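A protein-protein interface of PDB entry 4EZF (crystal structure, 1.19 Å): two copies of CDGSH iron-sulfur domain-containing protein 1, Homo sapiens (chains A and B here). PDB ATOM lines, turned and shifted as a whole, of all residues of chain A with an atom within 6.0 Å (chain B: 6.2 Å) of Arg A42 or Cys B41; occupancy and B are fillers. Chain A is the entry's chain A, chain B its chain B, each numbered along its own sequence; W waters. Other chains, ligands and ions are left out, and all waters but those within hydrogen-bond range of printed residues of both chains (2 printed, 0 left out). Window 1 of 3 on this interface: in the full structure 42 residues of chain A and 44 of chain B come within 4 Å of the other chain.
Of the 12 printed residues of chain A, 12 touch a printed residue of chain B.
Of the 22 printed residues of chain B, 15 touch a printed residue of chain A.
Hydrophobic or aromatic side chains of chain B that line the printed part of chain A: Ile B13, Ile B24, Val B25, His B26, Phe B28, Tyr B40, Trp B44, Phe B49, Pro B50 and Leu B70.
Among the printed residues, 28 pairs touch across the chains.
Among the printed residues, no Asp or Glu carboxylate lies within 4 Å of a Lys or Arg side-chain nitrogen of the other chain.
The guanidinium group (NH2) of Arg A42 lies within hydrogen-bond range of the backbone carbonyl oxygen (O) of Ile B24.
ND1 of His B26 sits at hydrogen-bond distance from NH1 of Arg A42.
NE1 of Trp B44 sits at hydrogen-bond distance from O of Arg A42 (2.8 Å).
O of Arg B42 sits at hydrogen-bond distance from NE1 of Trp A44 (2.8 Å).
N of Gly A68 lies within hydrogen-bond range of O of Ile B24.
The backbone NH (N) of His B26 is in hydrogen-bond range of the backbone carbonyl oxygen (O) of Pro A69, 3.3 Å away.
Ile A13 touches Cys B43 (CD1 to O, 3.1 Å).
NH2 of Arg A42 touches CA of Val B25, at 3.7 Å.
Arg A42 touches Phe B49 (NH1 to CZ, 3.5 Å).
Pro B50 touches Arg A42.
Cys A43 touches Ile B13 (O to CD1, 3.1 Å).
Phe A49 touches Arg B42 (CZ to NH1, 3.5 Å).
CB of Pro A50 touches NH1 of Arg B42 (3.8 Å).
Ile B24 touches Val A67.
Val A67 touches Trp B44.
Leu A70 touches Phe B28.
Water W1 lies within hydrogen-bond range of the backbone carbonyl oxygen (O) of Cys A41 (2.7 Å), the backbone carbonyl oxygen (O) of Pro A50 (2.8 Å) and the guanidinium group (NH1) of Arg B42 (2.8 Å).
Water W2 lies within hydrogen-bond range of the backbone carbonyl oxygen (O) of Cys B41, the guanidinium group (NH1) of Arg A42 and the backbone carbonyl oxygen (O) of Pro B50.
Arg A42 touches just these residues of chain B: Ile B24 (3.0 Å), Val B25 (3.7 Å), His B26 (3.1 Å), Cys B41 (3.6 Å), Arg B42 (3.8 Å), Trp B44 (2.8 Å), Phe B49 (3.5 Å) and Pro B50 (3.8 Å).
Of chain A, only Arg A42 (3.6 Å) comes within 4 Å of Cys B41.
Of the printed residues of chain A, Gly B68 touches Trp A44 (3.6 Å).
Of the printed residues of chain B, Trp A44 touches Arg B42 (2.8 Å) and Gly B68 (3.6 Å).
Printed residues of chain A within 4 Å of Leu B70: Tyr A40 (3.5 Å) and Leu A70 (3.6 Å).
Printed residues of chain A within 4 Å of Cys B43: Ile A13 (3.1 Å).
Asp B53 touches none of the printed residues of chain A.
The nearest residue of chain B that does not touch Arg A42 is Ile B13 (4.6 Å).
The nearest printed residue of chain A that does not touch Val B25 is Gly A68 (4.5 Å).
N of Cys A41 lies within hydrogen-bond range of O of Pro A50 (2.9 Å).
O of Gly A68 lies within hydrogen-bond range of NE of Arg A42, 2.8 Å away.
The guanidinium group of Arg B45 lies within hydrogen-bond range of the backbone carbonyl oxygen of Ile B13, 2.7 Å away.
The backbone NH of Cys B41 sits at hydrogen-bond distance from the backbone carbonyl oxygen of Pro B50, 2.9 Å away.
The guanidinium group of Arg B42 is in hydrogen-bond range of the backbone carbonyl oxygen of Gly B68.
O of Cys B43 is in hydrogen-bond range of NH1 of Arg B45 (3.3 Å).
Ile A13 touches Cys B43, and with the chains exchanged Cys A43 touches Ile B13.
Arg A42 touches Phe B49, and with the chains exchanged Phe A49 touches Arg B42.
Arg A42 touches Pro B50, and with the chains exchanged Pro A50 touches Arg B42.
Leu A70 touches its own counterpart, Leu B70.
Positions printed for both chains: 13, 40, 41, 42, 43, 44, 49, 50, 68, 69 and 70.
Of the 28 pairs that touch across the chains among the printed residues, 17 have their exchanged pair printed and touching as well.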
ATOM      1  N   ILE A  13     -13.845  -8.276  31.180  1.00  0.00           N
ATOM      2  CA  ILE A  13     -14.735  -9.393  30.845  1.00  0.00           C
ATOM      3  C   ILE A  13     -13.947 -10.586  30.347  1.00  0.00           C
ATOM      4  O   ILE A  13     -14.126 -11.700  30.859  1.00  0.00           O
ATOM      5  CB  ILE A  13     -15.788  -8.946  29.822  1.00  0.00           C
ATOM      6  CG1 ILE A  13     -16.760  -7.981  30.505  1.00  0.00           C
ATOM      7  CG2 ILE A  13     -16.504 -10.139  29.181  1.00  0.00           C
ATOM      8  CD1 ILE A  13     -17.673  -7.286  29.547  1.00  0.00           C
ATOM      9  N   TYR A  40     -23.082 -19.742  20.190  1.00  0.00           N
ATOM     10  CA  TYR A  40     -21.934 -18.847  20.352  1.00  0.00           C
ATOM     11  C   TYR A  40     -21.799 -18.367  21.782  1.00  0.00           C
ATOM     12  O   TYR A  40     -22.789 -17.995  22.426  1.00  0.00           O
ATOM     13  CB  TYR A  40     -22.051 -17.638  19.430  1.00  0.00           C
ATOM     14  CG  TYR A  40     -22.022 -18.005  17.975  1.00  0.00           C
ATOM     15  CD1 TYR A  40     -20.852 -18.469  17.374  1.00  0.00           C
ATOM     16  CD2 TYR A  40     -23.160 -17.863  17.176  1.00  0.00           C
ATOM     17  CE1 TYR A  40     -20.818 -18.797  16.027  1.00  0.00           C
ATOM     18  CE2 TYR A  40     -23.143 -18.181  15.832  1.00  0.00           C
ATOM     19  CZ  TYR A  40     -21.961 -18.642  15.259  1.00  0.00           C
ATOM     20  OH  TYR A  40     -21.957 -18.961  13.921  1.00  0.00           O
ATOM     21  N   CYS A  41     -20.575 -18.378  22.286  1.00  0.00           N
ATOM     22  CA  CYS A  41     -20.250 -17.961  23.641  1.00  0.00           C
ATOM     23  C   CYS A  41     -20.340 -16.445  23.798  1.00  0.00           C
ATOM     24  O   CYS A  41     -19.770 -15.687  22.981  1.00  0.00           O
ATOM     25  CB  CYS A  41     -18.837 -18.444  24.021  1.00  0.00           C
ATOM     26  SG  CYS A  41     -18.285 -17.981  25.645  1.00  0.00           S
ATOM     27  N   ARG A  42     -21.033 -15.989  24.839  1.00  0.00           N
ATOM     28  CA  ARG A  42     -21.073 -14.588  25.217  1.00  0.00           C
ATOM     29  C   ARG A  42     -20.433 -14.359  26.589  1.00  0.00           C
ATOM     30  O   ARG A  42     -20.552 -13.267  27.134  1.00  0.00           O
ATOM     31  CB  ARG A  42     -22.504 -14.030  25.150  1.00  0.00           C
ATOM     32  CG  ARG A  42     -23.111 -14.141  23.786  1.00  0.00           C
ATOM     33  CD  ARG A  42     -24.405 -13.358  23.626  1.00  0.00           C
ATOM     34  NE  ARG A  42     -25.478 -13.951  24.438  1.00  0.00           N
ATOM     35  CZ  ARG A  42     -26.761 -13.594  24.352  1.00  0.00           C
ATOM     36  NH1 ARG A  42     -27.169 -12.720  23.441  1.00  0.00           N
ATOM     37  NH2 ARG A  42     -27.666 -14.134  25.168  1.00  0.00           N
ATOM     38  N   CYS A  43     -19.722 -15.342  27.143  1.00  0.00           N
ATOM     39  CA  CYS A  43     -19.157 -15.200  28.481  1.00  0.00           C
ATOM     40  C   CYS A  43     -17.641 -15.190  28.500  1.00  0.00           C
ATOM     41  O   CYS A  43     -17.043 -14.937  29.543  1.00  0.00           O
ATOM     42  CB  CYS A  43     -19.650 -16.297  29.438  1.00  0.00           C
ATOM     43  SG  CYS A  43     -18.923 -17.965  29.183  1.00  0.00           S
ATOM     44  N   TRP A  44     -17.009 -15.500  27.367  1.00  0.00           N
ATOM     45  CA  TRP A  44     -15.542 -15.427  27.295  1.00  0.00           C
ATOM     46  C   TRP A  44     -14.871 -16.401  28.269  1.00  0.00           C
ATOM     47  O   TRP A  44     -13.714 -16.183  28.671  1.00  0.00           O
ATOM     48  CB  TRP A  44     -15.043 -13.975  27.482  1.00  0.00           C
ATOM     49  CG  TRP A  44     -15.642 -13.050  26.485  1.00  0.00           C
ATOM     50  CD1 TRP A  44     -16.854 -12.453  26.576  1.00  0.00           C
ATOM     51  CD2 TRP A  44     -15.104 -12.664  25.203  1.00  0.00           C
ATOM     52  NE1 TRP A  44     -17.124 -11.717  25.452  1.00  0.00           N
ATOM     53  CE2 TRP A  44     -16.060 -11.817  24.592  1.00  0.00           C
ATOM     54  CE3 TRP A  44     -13.900 -12.925  24.533  1.00  0.00           C
ATOM     55  CZ2 TRP A  44     -15.873 -11.262  23.330  1.00  0.00           C
ATOM     56  CZ3 TRP A  44     -13.703 -12.348  23.288  1.00  0.00           C
ATOM     57  CH2 TRP A  44     -14.665 -11.509  22.706  1.00  0.00           C
ATOM     58  N   PHE A  49     -14.044 -21.116  22.546  1.00  0.00           N
ATOM     59  CA  PHE A  49     -14.449 -19.798  22.050  1.00  0.00           C
ATOM     60  C   PHE A  49     -14.068 -19.702  20.582  1.00  0.00           C
ATOM     61  O   PHE A  49     -12.956 -20.065  20.242  1.00  0.00           O
ATOM     62  CB  PHE A  49     -13.749 -18.696  22.843  1.00  0.00           C
ATOM     63  CG  PHE A  49     -14.408 -17.362  22.696  1.00  0.00           C
ATOM     64  CD1 PHE A  49     -15.524 -17.048  23.470  1.00  0.00           C
ATOM     65  CD2 PHE A  49     -13.963 -16.442  21.757  1.00  0.00           C
ATOM     66  CE1 PHE A  49     -16.166 -15.847  23.322  1.00  0.00           C
ATOM     67  CE2 PHE A  49     -14.601 -15.237  21.606  1.00  0.00           C
ATOM     68  CZ  PHE A  49     -15.707 -14.925  22.398  1.00  0.00           C
ATOM     69  N   PRO A  50     -14.941 -19.196  19.695  1.00  0.00           N
ATOM     70  CA  PRO A  50     -16.181 -18.448  19.973  1.00  0.00           C
ATOM     71  C   PRO A  50     -17.438 -19.299  20.192  1.00  0.00           C
ATOM     72  O   PRO A  50     -18.534 -18.721  20.281  1.00  0.00           O
ATOM     73  CB  PRO A  50     -16.342 -17.617  18.701  1.00  0.00           C
ATOM     74  CG  PRO A  50     -15.772 -18.525  17.628  1.00  0.00           C
ATOM     75  CD  PRO A  50     -14.599 -19.198  18.250  1.00  0.00           C
ATOM     76  N   VAL A  67     -25.383 -14.744  32.554  1.00  0.00           N
ATOM     77  CA  VAL A  67     -25.095 -14.680  31.118  1.00  0.00           C
ATOM     78  C   VAL A  67     -25.292 -16.040  30.446  1.00  0.00           C
ATOM     79  O   VAL A  67     -25.229 -17.094  31.096  1.00  0.00           O
ATOM     80  CB  VAL A  67     -23.676 -14.128  30.833  1.00  0.00           C
ATOM     81  CG1 VAL A  67     -23.626 -12.666  31.249  1.00  0.00           C
ATOM     82  CG2 VAL A  67     -22.611 -14.969  31.538  1.00  0.00           C
ATOM     83  N   GLY A  68     -25.538 -16.024  29.146  1.00  0.00           N
ATOM     84  CA  GLY A  68     -25.691 -17.260  28.410  1.00  0.00           C
ATOM     85  C   GLY A  68     -25.455 -17.002  26.938  1.00  0.00           C
ATOM     86  O   GLY A  68     -25.211 -15.858  26.529  1.00  0.00           O
ATOM     87  N   PRO A  69     -25.548 -18.054  26.131  1.00  0.00           N
ATOM     88  CA  PRO A  69     -25.106 -17.998  24.729  1.00  0.00           C
ATOM     89  C   PRO A  69     -26.126 -17.408  23.764  1.00  0.00           C
ATOM     90  O   PRO A  69     -27.296 -17.100  24.102  1.00  0.00           O
ATOM     91  CB  PRO A  69     -24.829 -19.471  24.391  1.00  0.00           C
ATOM     92  CG  PRO A  69     -25.832 -20.219  25.287  1.00  0.00           C
ATOM     93  CD  PRO A  69     -25.738 -19.446  26.586  1.00  0.00           C
ATOM     94  N   LEU A  70     -25.649 -17.290  22.524  1.00  0.00           N
ATOM     95  CA  LEU A  70     -26.418 -16.828  21.388  1.00  0.00           C
ATOM     96  C   LEU A  70     -26.565 -18.000  20.428  1.00  0.00           C
ATOM     97  O   LEU A  70     -25.562 -18.538  19.955  1.00  0.00           O
ATOM     98  CB  LEU A  70     -25.647 -15.687  20.694  1.00  0.00           C
ATOM     99  CG  LEU A  70     -26.223 -15.165  19.387  1.00  0.00           C
ATOM    100  CD1 LEU A  70     -27.517 -14.394  19.584  1.00  0.00           C
ATOM    101  CD2 LEU A  70     -25.167 -14.291  18.699  1.00  0.00           C
ATOM    102  N   ILE B  13     -19.900 -10.417  34.554  1.00  0.00           N
ATOM    103  CA  ILE B  13     -19.710  -9.885  33.220  1.00  0.00           C
ATOM    104  C   ILE B  13     -20.857  -8.944  32.890  1.00  0.00           C
ATOM    105  O   ILE B  13     -20.635  -7.824  32.452  1.00  0.00           O
ATOM    106  CB  ILE B  13     -19.650 -11.038  32.213  1.00  0.00           C
ATOM    107  CG1 ILE B  13     -18.316 -11.766  32.381  1.00  0.00           C
ATOM    108  CG2 ILE B  13     -19.900 -10.553  30.780  1.00  0.00           C
ATOM    109  CD1 ILE B  13     -18.286 -13.080  31.681  1.00  0.00           C
ATOM    110  N   ILE B  17     -28.197  -5.964  32.633  1.00  0.00           N
ATOM    111  CA  ILE B  17     -29.183  -6.362  31.645  1.00  0.00           C
ATOM    112  C   ILE B  17     -30.078  -7.494  32.157  1.00  0.00           C
ATOM    113  O   ILE B  17     -29.574  -8.527  32.614  1.00  0.00           O
ATOM    114  CB  ILE B  17     -28.485  -6.756  30.326  1.00  0.00           C
ATOM    115  CG1 ILE B  17     -27.718  -5.556  29.744  1.00  0.00           C
ATOM    116  CG2 ILE B  17     -29.487  -7.306  29.311  1.00  0.00           C
ATOM    117  CD1 ILE B  17     -26.761  -5.956  28.630  1.00  0.00           C
ATOM    118  N   ILE B  24     -29.514 -15.479  30.513  1.00  0.00           N
ATOM    119  CA  ILE B  24     -29.955 -14.803  29.308  1.00  0.00           C
ATOM    120  C   ILE B  24     -29.418 -15.494  28.054  1.00  0.00           C
ATOM    121  O   ILE B  24     -28.216 -15.478  27.786  1.00  0.00           O
ATOM    122  CB  ILE B  24     -29.563 -13.316  29.337  1.00  0.00           C
ATOM    123  CG1 ILE B  24     -30.206 -12.586  30.533  1.00  0.00           C
ATOM    124  CG2 ILE B  24     -29.891 -12.648  28.015  1.00  0.00           C
ATOM    125  CD1 ILE B  24     -29.512 -11.246  30.832  1.00  0.00           C
ATOM    126  N   VAL B  25     -30.331 -16.080  27.299  1.00  0.00           N
ATOM    127  CA  VAL B  25     -30.076 -16.770  26.044  1.00  0.00           C
ATOM    128  C   VAL B  25     -30.924 -16.138  24.962  1.00  0.00           C
ATOM    129  O   VAL B  25     -32.104 -15.829  25.203  1.00  0.00           O
ATOM    130  CB  VAL B  25     -30.442 -18.265  26.172  1.00  0.00           C
ATOM    131  CG1 VAL B  25     -30.102 -19.051  24.908  1.00  0.00           C
ATOM    132  CG2 VAL B  25     -29.734 -18.864  27.371  1.00  0.00           C
ATOM    133  N   HIS B  26     -30.325 -15.914  23.789  1.00  0.00           N
ATOM    134  CA  HIS B  26     -31.091 -15.487  22.629  1.00  0.00           C
ATOM    135  C   HIS B  26     -30.964 -16.514  21.539  1.00  0.00           C
ATOM    136  O   HIS B  26     -29.885 -17.052  21.332  1.00  0.00           O
ATOM    137  CB  HIS B  26     -30.652 -14.129  22.124  1.00  0.00           C
ATOM    138  CG  HIS B  26     -31.001 -13.018  23.047  1.00  0.00           C
ATOM    139  ND1 HIS B  26     -30.209 -12.644  24.118  1.00  0.00           N
ATOM    140  CD2 HIS B  26     -32.089 -12.214  23.072  1.00  0.00           C
ATOM    141  CE1 HIS B  26     -30.800 -11.643  24.757  1.00  0.00           C
ATOM    142  NE2 HIS B  26     -31.942 -11.367  24.143  1.00  0.00           N
ATOM    143  N   PHE B  28     -32.033 -17.055  17.399  1.00  0.00           N
ATOM    144  CA  PHE B  28     -32.554 -16.505  16.172  1.00  0.00           C
ATOM    145  C   PHE B  28     -32.383 -17.507  15.038  1.00  0.00           C
ATOM    146  O   PHE B  28     -31.403 -18.256  14.972  1.00  0.00           O
ATOM    147  CB  PHE B  28     -31.801 -15.221  15.788  1.00  0.00           C
ATOM    148  CG  PHE B  28     -31.917 -14.118  16.805  1.00  0.00           C
ATOM    149  CD1 PHE B  28     -33.088 -13.379  16.894  1.00  0.00           C
ATOM    150  CD2 PHE B  28     -30.893 -13.831  17.682  1.00  0.00           C
ATOM    151  CE1 PHE B  28     -33.240 -12.361  17.831  1.00  0.00           C
ATOM    152  CE2 PHE B  28     -31.026 -12.809  18.617  1.00  0.00           C
ATOM    153  CZ  PHE B  28     -32.197 -12.067  18.690  1.00  0.00           C
ATOM    154  N   VAL B  39     -25.215  -7.873  13.878  1.00  0.00           N
ATOM    155  CA  VAL B  39     -24.033  -7.694  14.717  1.00  0.00           C
ATOM    156  C   VAL B  39     -24.469  -7.806  16.181  1.00  0.00           C
ATOM    157  O   VAL B  39     -25.215  -6.957  16.693  1.00  0.00           O
ATOM    158  CB  VAL B  39     -23.331  -6.336  14.465  1.00  0.00           C
ATOM    159  CG1 VAL B  39     -22.031  -6.278  15.228  1.00  0.00           C
ATOM    160  CG2 VAL B  39     -23.035  -6.143  12.972  1.00  0.00           C
ATOM    161  N   TYR B  40     -24.017  -8.875  16.831  1.00  0.00           N
ATOM    162  CA  TYR B  40     -24.497  -9.250  18.163  1.00  0.00           C
ATOM    163  C   TYR B  40     -23.476  -8.914  19.238  1.00  0.00           C
ATOM    164  O   TYR B  40     -22.276  -9.163  19.095  1.00  0.00           O
ATOM    165  CB  TYR B  40     -24.809 -10.739  18.177  1.00  0.00           C
ATOM    166  CG  TYR B  40     -25.909 -11.142  17.228  1.00  0.00           C
ATOM    167  CD1 TYR B  40     -27.249 -10.920  17.552  1.00  0.00           C
ATOM    168  CD2 TYR B  40     -25.617 -11.790  16.033  1.00  0.00           C
ATOM    169  CE1 TYR B  40     -28.247 -11.308  16.689  1.00  0.00           C
ATOM    170  CE2 TYR B  40     -26.623 -12.198  15.181  1.00  0.00           C
ATOM    171  CZ  TYR B  40     -27.940 -11.946  15.504  1.00  0.00           C
ATOM    172  OH  TYR B  40     -28.916 -12.367  14.623  1.00  0.00           O
ATOM    173  N   CYS B  41     -23.955  -8.354  20.335  1.00  0.00           N
ATOM    174  CA  CYS B  41     -23.116  -7.937  21.450  1.00  0.00           C
ATOM    175  C   CYS B  41     -22.579  -9.117  22.266  1.00  0.00           C
ATOM    176  O   CYS B  41     -23.345 -10.021  22.647  1.00  0.00           O
ATOM    177  CB  CYS B  41     -23.899  -6.987  22.355  1.00  0.00           C
ATOM    178  SG  CYS B  41     -23.045  -6.381  23.810  1.00  0.00           S
ATOM    179  N   ARG B  42     -21.282  -9.078  22.576  1.00  0.00           N
ATOM    180  CA  ARG B  42     -20.658 -10.041  23.477  1.00  0.00           C
ATOM    181  C   ARG B  42     -20.081  -9.376  24.724  1.00  0.00           C
ATOM    182  O   ARG B  42     -19.374 -10.042  25.490  1.00  0.00           O
ATOM    183  CB  ARG B  42     -19.590 -10.866  22.745  1.00  0.00           C
ATOM    184  CG  ARG B  42     -20.146 -11.682  21.580  1.00  0.00           C
ATOM    185  CD  ARG B  42     -19.157 -12.701  21.034  1.00  0.00           C
ATOM    186  NE  ARG B  42     -17.997 -12.026  20.417  1.00  0.00           N
ATOM    187  CZ  ARG B  42     -17.094 -12.652  19.667  1.00  0.00           C
ATOM    188  NH1 ARG B  42     -17.223 -13.947  19.361  1.00  0.00           N
ATOM    189  NH2 ARG B  42     -16.049 -11.987  19.172  1.00  0.00           N
ATOM    190  N   CYS B  43     -20.372  -8.090  24.937  1.00  0.00           N
ATOM    191  CA  CYS B  43     -19.791  -7.352  26.061  1.00  0.00           C
ATOM    192  C   CYS B  43     -20.809  -7.016  27.149  1.00  0.00           C
ATOM    193  O   CYS B  43     -20.418  -6.560  28.223  1.00  0.00           O
ATOM    194  CB  CYS B  43     -19.077  -6.074  25.590  1.00  0.00           C
ATOM    195  SG  CYS B  43     -20.160  -4.707  25.146  1.00  0.00           S
ATOM    196  N   TRP B  44     -22.102  -7.179  26.861  1.00  0.00           N
ATOM    197  CA  TRP B  44     -23.157  -6.928  27.866  1.00  0.00           C
ATOM    198  C   TRP B  44     -23.181  -5.468  28.307  1.00  0.00           C
ATOM    199  O   TRP B  44     -23.632  -5.168  29.411  1.00  0.00           O
ATOM    200  CB  TRP B  44     -23.029  -7.893  29.071  1.00  0.00           C
ATOM    201  CG  TRP B  44     -23.095  -9.334  28.624  1.00  0.00           C
ATOM    202  CD1 TRP B  44     -22.065 -10.074  28.131  1.00  0.00           C
ATOM    203  CD2 TRP B  44     -24.259 -10.173  28.546  1.00  0.00           C
ATOM    204  NE1 TRP B  44     -22.489 -11.323  27.741  1.00  0.00           N
ATOM    205  CE2 TRP B  44     -23.839 -11.420  28.004  1.00  0.00           C
ATOM    206  CE3 TRP B  44     -25.611 -10.013  28.908  1.00  0.00           C
ATOM    207  CZ2 TRP B  44     -24.711 -12.478  27.793  1.00  0.00           C
ATOM    208  CZ3 TRP B  44     -26.475 -11.082  28.698  1.00  0.00           C
ATOM    209  CH2 TRP B  44     -26.023 -12.297  28.165  1.00  0.00           C
ATOM    210  N   ARG B  45     -22.713  -4.563  27.446  1.00  0.00           N
ATOM    211  CA  ARG B  45     -22.800  -3.132  27.745  1.00  0.00           C
ATOM    212  C   ARG B  45     -23.685  -2.384  26.741  1.00  0.00           C
ATOM    213  O   ARG B  45     -23.984  -1.211  26.941  1.00  0.00           O
ATOM    214  CB  ARG B  45     -21.409  -2.477  27.756  1.00  0.00           C
ATOM    215  CG  ARG B  45     -20.429  -3.072  28.740  1.00  0.00           C
ATOM    216  CD  ARG B  45     -20.856  -2.785  30.178  1.00  0.00           C
ATOM    217  NE  ARG B  45     -19.913  -3.366  31.118  1.00  0.00           N
ATOM    218  CZ  ARG B  45     -19.990  -4.606  31.596  1.00  0.00           C
ATOM    219  NH1 ARG B  45     -21.001  -5.405  31.276  1.00  0.00           N
ATOM    220  NH2 ARG B  45     -19.061  -5.047  32.424  1.00  0.00           N
ATOM    221  N   SER B  46     -24.085  -3.030  25.656  1.00  0.00           N
ATOM    222  CA  SER B  46     -24.943  -2.382  24.679  1.00  0.00           C
ATOM    223  C   SER B  46     -26.272  -1.967  25.297  1.00  0.00           C
ATOM    224  O   SER B  46     -26.827  -2.669  26.150  1.00  0.00           O
ATOM    225  CB  SER B  46     -25.231  -3.315  23.518  1.00  0.00           C
ATOM    226  OG  SER B  46     -26.085  -2.657  22.598  1.00  0.00           O
ATOM    227  N   PHE B  49     -28.942  -4.426  23.600  1.00  0.00           N
ATOM    228  CA  PHE B  49     -28.673  -5.857  23.737  1.00  0.00           C
ATOM    229  C   PHE B  49     -29.911  -6.622  23.293  1.00  0.00           C
ATOM    230  O   PHE B  49     -31.009  -6.273  23.714  1.00  0.00           O
ATOM    231  CB  PHE B  49     -28.306  -6.202  25.193  1.00  0.00           C
ATOM    232  CG  PHE B  49     -27.602  -7.523  25.336  1.00  0.00           C
ATOM    233  CD1 PHE B  49     -26.238  -7.612  25.076  1.00  0.00           C
ATOM    234  CD2 PHE B  49     -28.295  -8.682  25.656  1.00  0.00           C
ATOM    235  CE1 PHE B  49     -25.588  -8.829  25.140  1.00  0.00           C
ATOM    236  CE2 PHE B  49     -27.645  -9.895  25.720  1.00  0.00           C
ATOM    237  CZ  PHE B  49     -26.294  -9.975  25.481  1.00  0.00           C
ATOM    238  N   PRO B  50     -29.763  -7.681  22.483  1.00  0.00           N
ATOM    239  CA  PRO B  50     -28.549  -8.437  22.169  1.00  0.00           C
ATOM    240  C   PRO B  50     -27.735  -7.915  20.978  1.00  0.00           C
ATOM    241  O   PRO B  50     -26.795  -8.582  20.554  1.00  0.00           O
ATOM    242  CB  PRO B  50     -29.122  -9.824  21.851  1.00  0.00           C
ATOM    243  CG  PRO B  50     -30.400  -9.504  21.140  1.00  0.00           C
ATOM    244  CD  PRO B  50     -30.967  -8.338  21.920  1.00  0.00           C
ATOM    245  N   PHE B  51     -28.070  -6.742  20.464  1.00  0.00           N
ATOM    246  CA  PHE B  51     -27.349  -6.184  19.318  1.00  0.00           C
ATOM    247  C   PHE B  51     -26.235  -5.255  19.766  1.00  0.00           C
ATOM    248  O   PHE B  51     -26.343  -4.603  20.782  1.00  0.00           O
ATOM    249  CB  PHE B  51     -28.337  -5.467  18.416  1.00  0.00           C
ATOM    250  CG  PHE B  51     -29.378  -6.386  17.924  1.00  0.00           C
ATOM    251  CD1 PHE B  51     -29.066  -7.338  16.969  1.00  0.00           C
ATOM    252  CD2 PHE B  51     -30.646  -6.390  18.477  1.00  0.00           C
ATOM    253  CE1 PHE B  51     -30.004  -8.242  16.531  1.00  0.00           C
ATOM    254  CE2 PHE B  51     -31.592  -7.301  18.042  1.00  0.00           C
ATOM    255  CZ  PHE B  51     -31.263  -8.223  17.072  1.00  0.00           C
ATOM    256  N   CYS B  52     -25.137  -5.212  19.020  1.00  0.00           N
ATOM    257  CA  CYS B  52     -23.998  -4.355  19.324  1.00  0.00           C
ATOM    258  C   CYS B  52     -24.302  -2.915  18.949  1.00  0.00           C
ATOM    259  O   CYS B  52     -24.818  -2.653  17.855  1.00  0.00           O
ATOM    260  CB  CYS B  52     -22.797  -4.859  18.502  1.00  0.00           C
ATOM    261  SG  CYS B  52     -21.282  -3.856  18.573  1.00  0.00           S
ATOM    262  N   ASP B  53     -23.990  -1.979  19.844  1.00  0.00           N
ATOM    263  CA  ASP B  53     -24.118  -0.537  19.565  1.00  0.00           C
ATOM    264  C   ASP B  53     -22.779   0.193  19.712  1.00  0.00           C
ATOM    265  O   ASP B  53     -22.747   1.419  19.794  1.00  0.00           O
ATOM    266  CB  ASP B  53     -25.203   0.122  20.446  1.00  0.00           C
ATOM    267  CG  ASP B  53     -24.819   0.181  21.918  1.00  0.00           C
ATOM    268  OD1 ASP B  53     -23.729  -0.316  22.281  1.00  0.00           O
ATOM    269  OD2 ASP B  53     -25.624   0.718  22.720  1.00  0.00           O
ATOM    270  N   GLY B  68     -15.267  -7.831  21.573  1.00  0.00           N
ATOM    271  CA  GLY B  68     -15.993  -7.293  20.449  1.00  0.00           C
ATOM    272  C   GLY B  68     -17.105  -8.232  20.043  1.00  0.00           C
ATOM    273  O   GLY B  68     -17.257  -9.317  20.660  1.00  0.00           O
ATOM    274  N   PRO B  69     -17.860  -7.846  19.010  1.00  0.00           N
ATOM    275  CA  PRO B  69     -19.102  -8.553  18.688  1.00  0.00           C
ATOM    276  C   PRO B  69     -18.941  -9.807  17.837  1.00  0.00           C
ATOM    277  O   PRO B  69     -17.838 -10.146  17.345  1.00  0.00           O
ATOM    278  CB  PRO B  69     -19.908  -7.502  17.928  1.00  0.00           C
ATOM    279  CG  PRO B  69     -18.837  -6.608  17.282  1.00  0.00           C
ATOM    280  CD  PRO B  69     -17.777  -6.530  18.357  1.00  0.00           C
ATOM    281  N   LEU B  70     -20.054 -10.515  17.692  1.00  0.00           N
ATOM    282  CA  LEU B  70     -20.164 -11.606  16.744  1.00  0.00           C
ATOM    283  C   LEU B  70     -21.060 -11.136  15.621  1.00  0.00           C
ATOM    284  O   LEU B  70     -22.175 -10.658  15.857  1.00  0.00           O
ATOM    285  CB  LEU B  70     -20.772 -12.848  17.378  1.00  0.00           C
ATOM    286  CG  LEU B  70     -21.048 -13.874  16.268  1.00  0.00           C
ATOM    287  CD1 LEU B  70     -19.962 -14.923  16.177  1.00  0.00           C
ATOM    288  CD2 LEU B  70     -22.406 -14.500  16.421  1.00  0.00           C
HETATM  289  O   HOH W   1     -18.993 -15.918  20.397  1.00  0.00           O
HETATM  290  O   HOH W   2     -25.735 -10.983  21.698  1.00  0.00           O
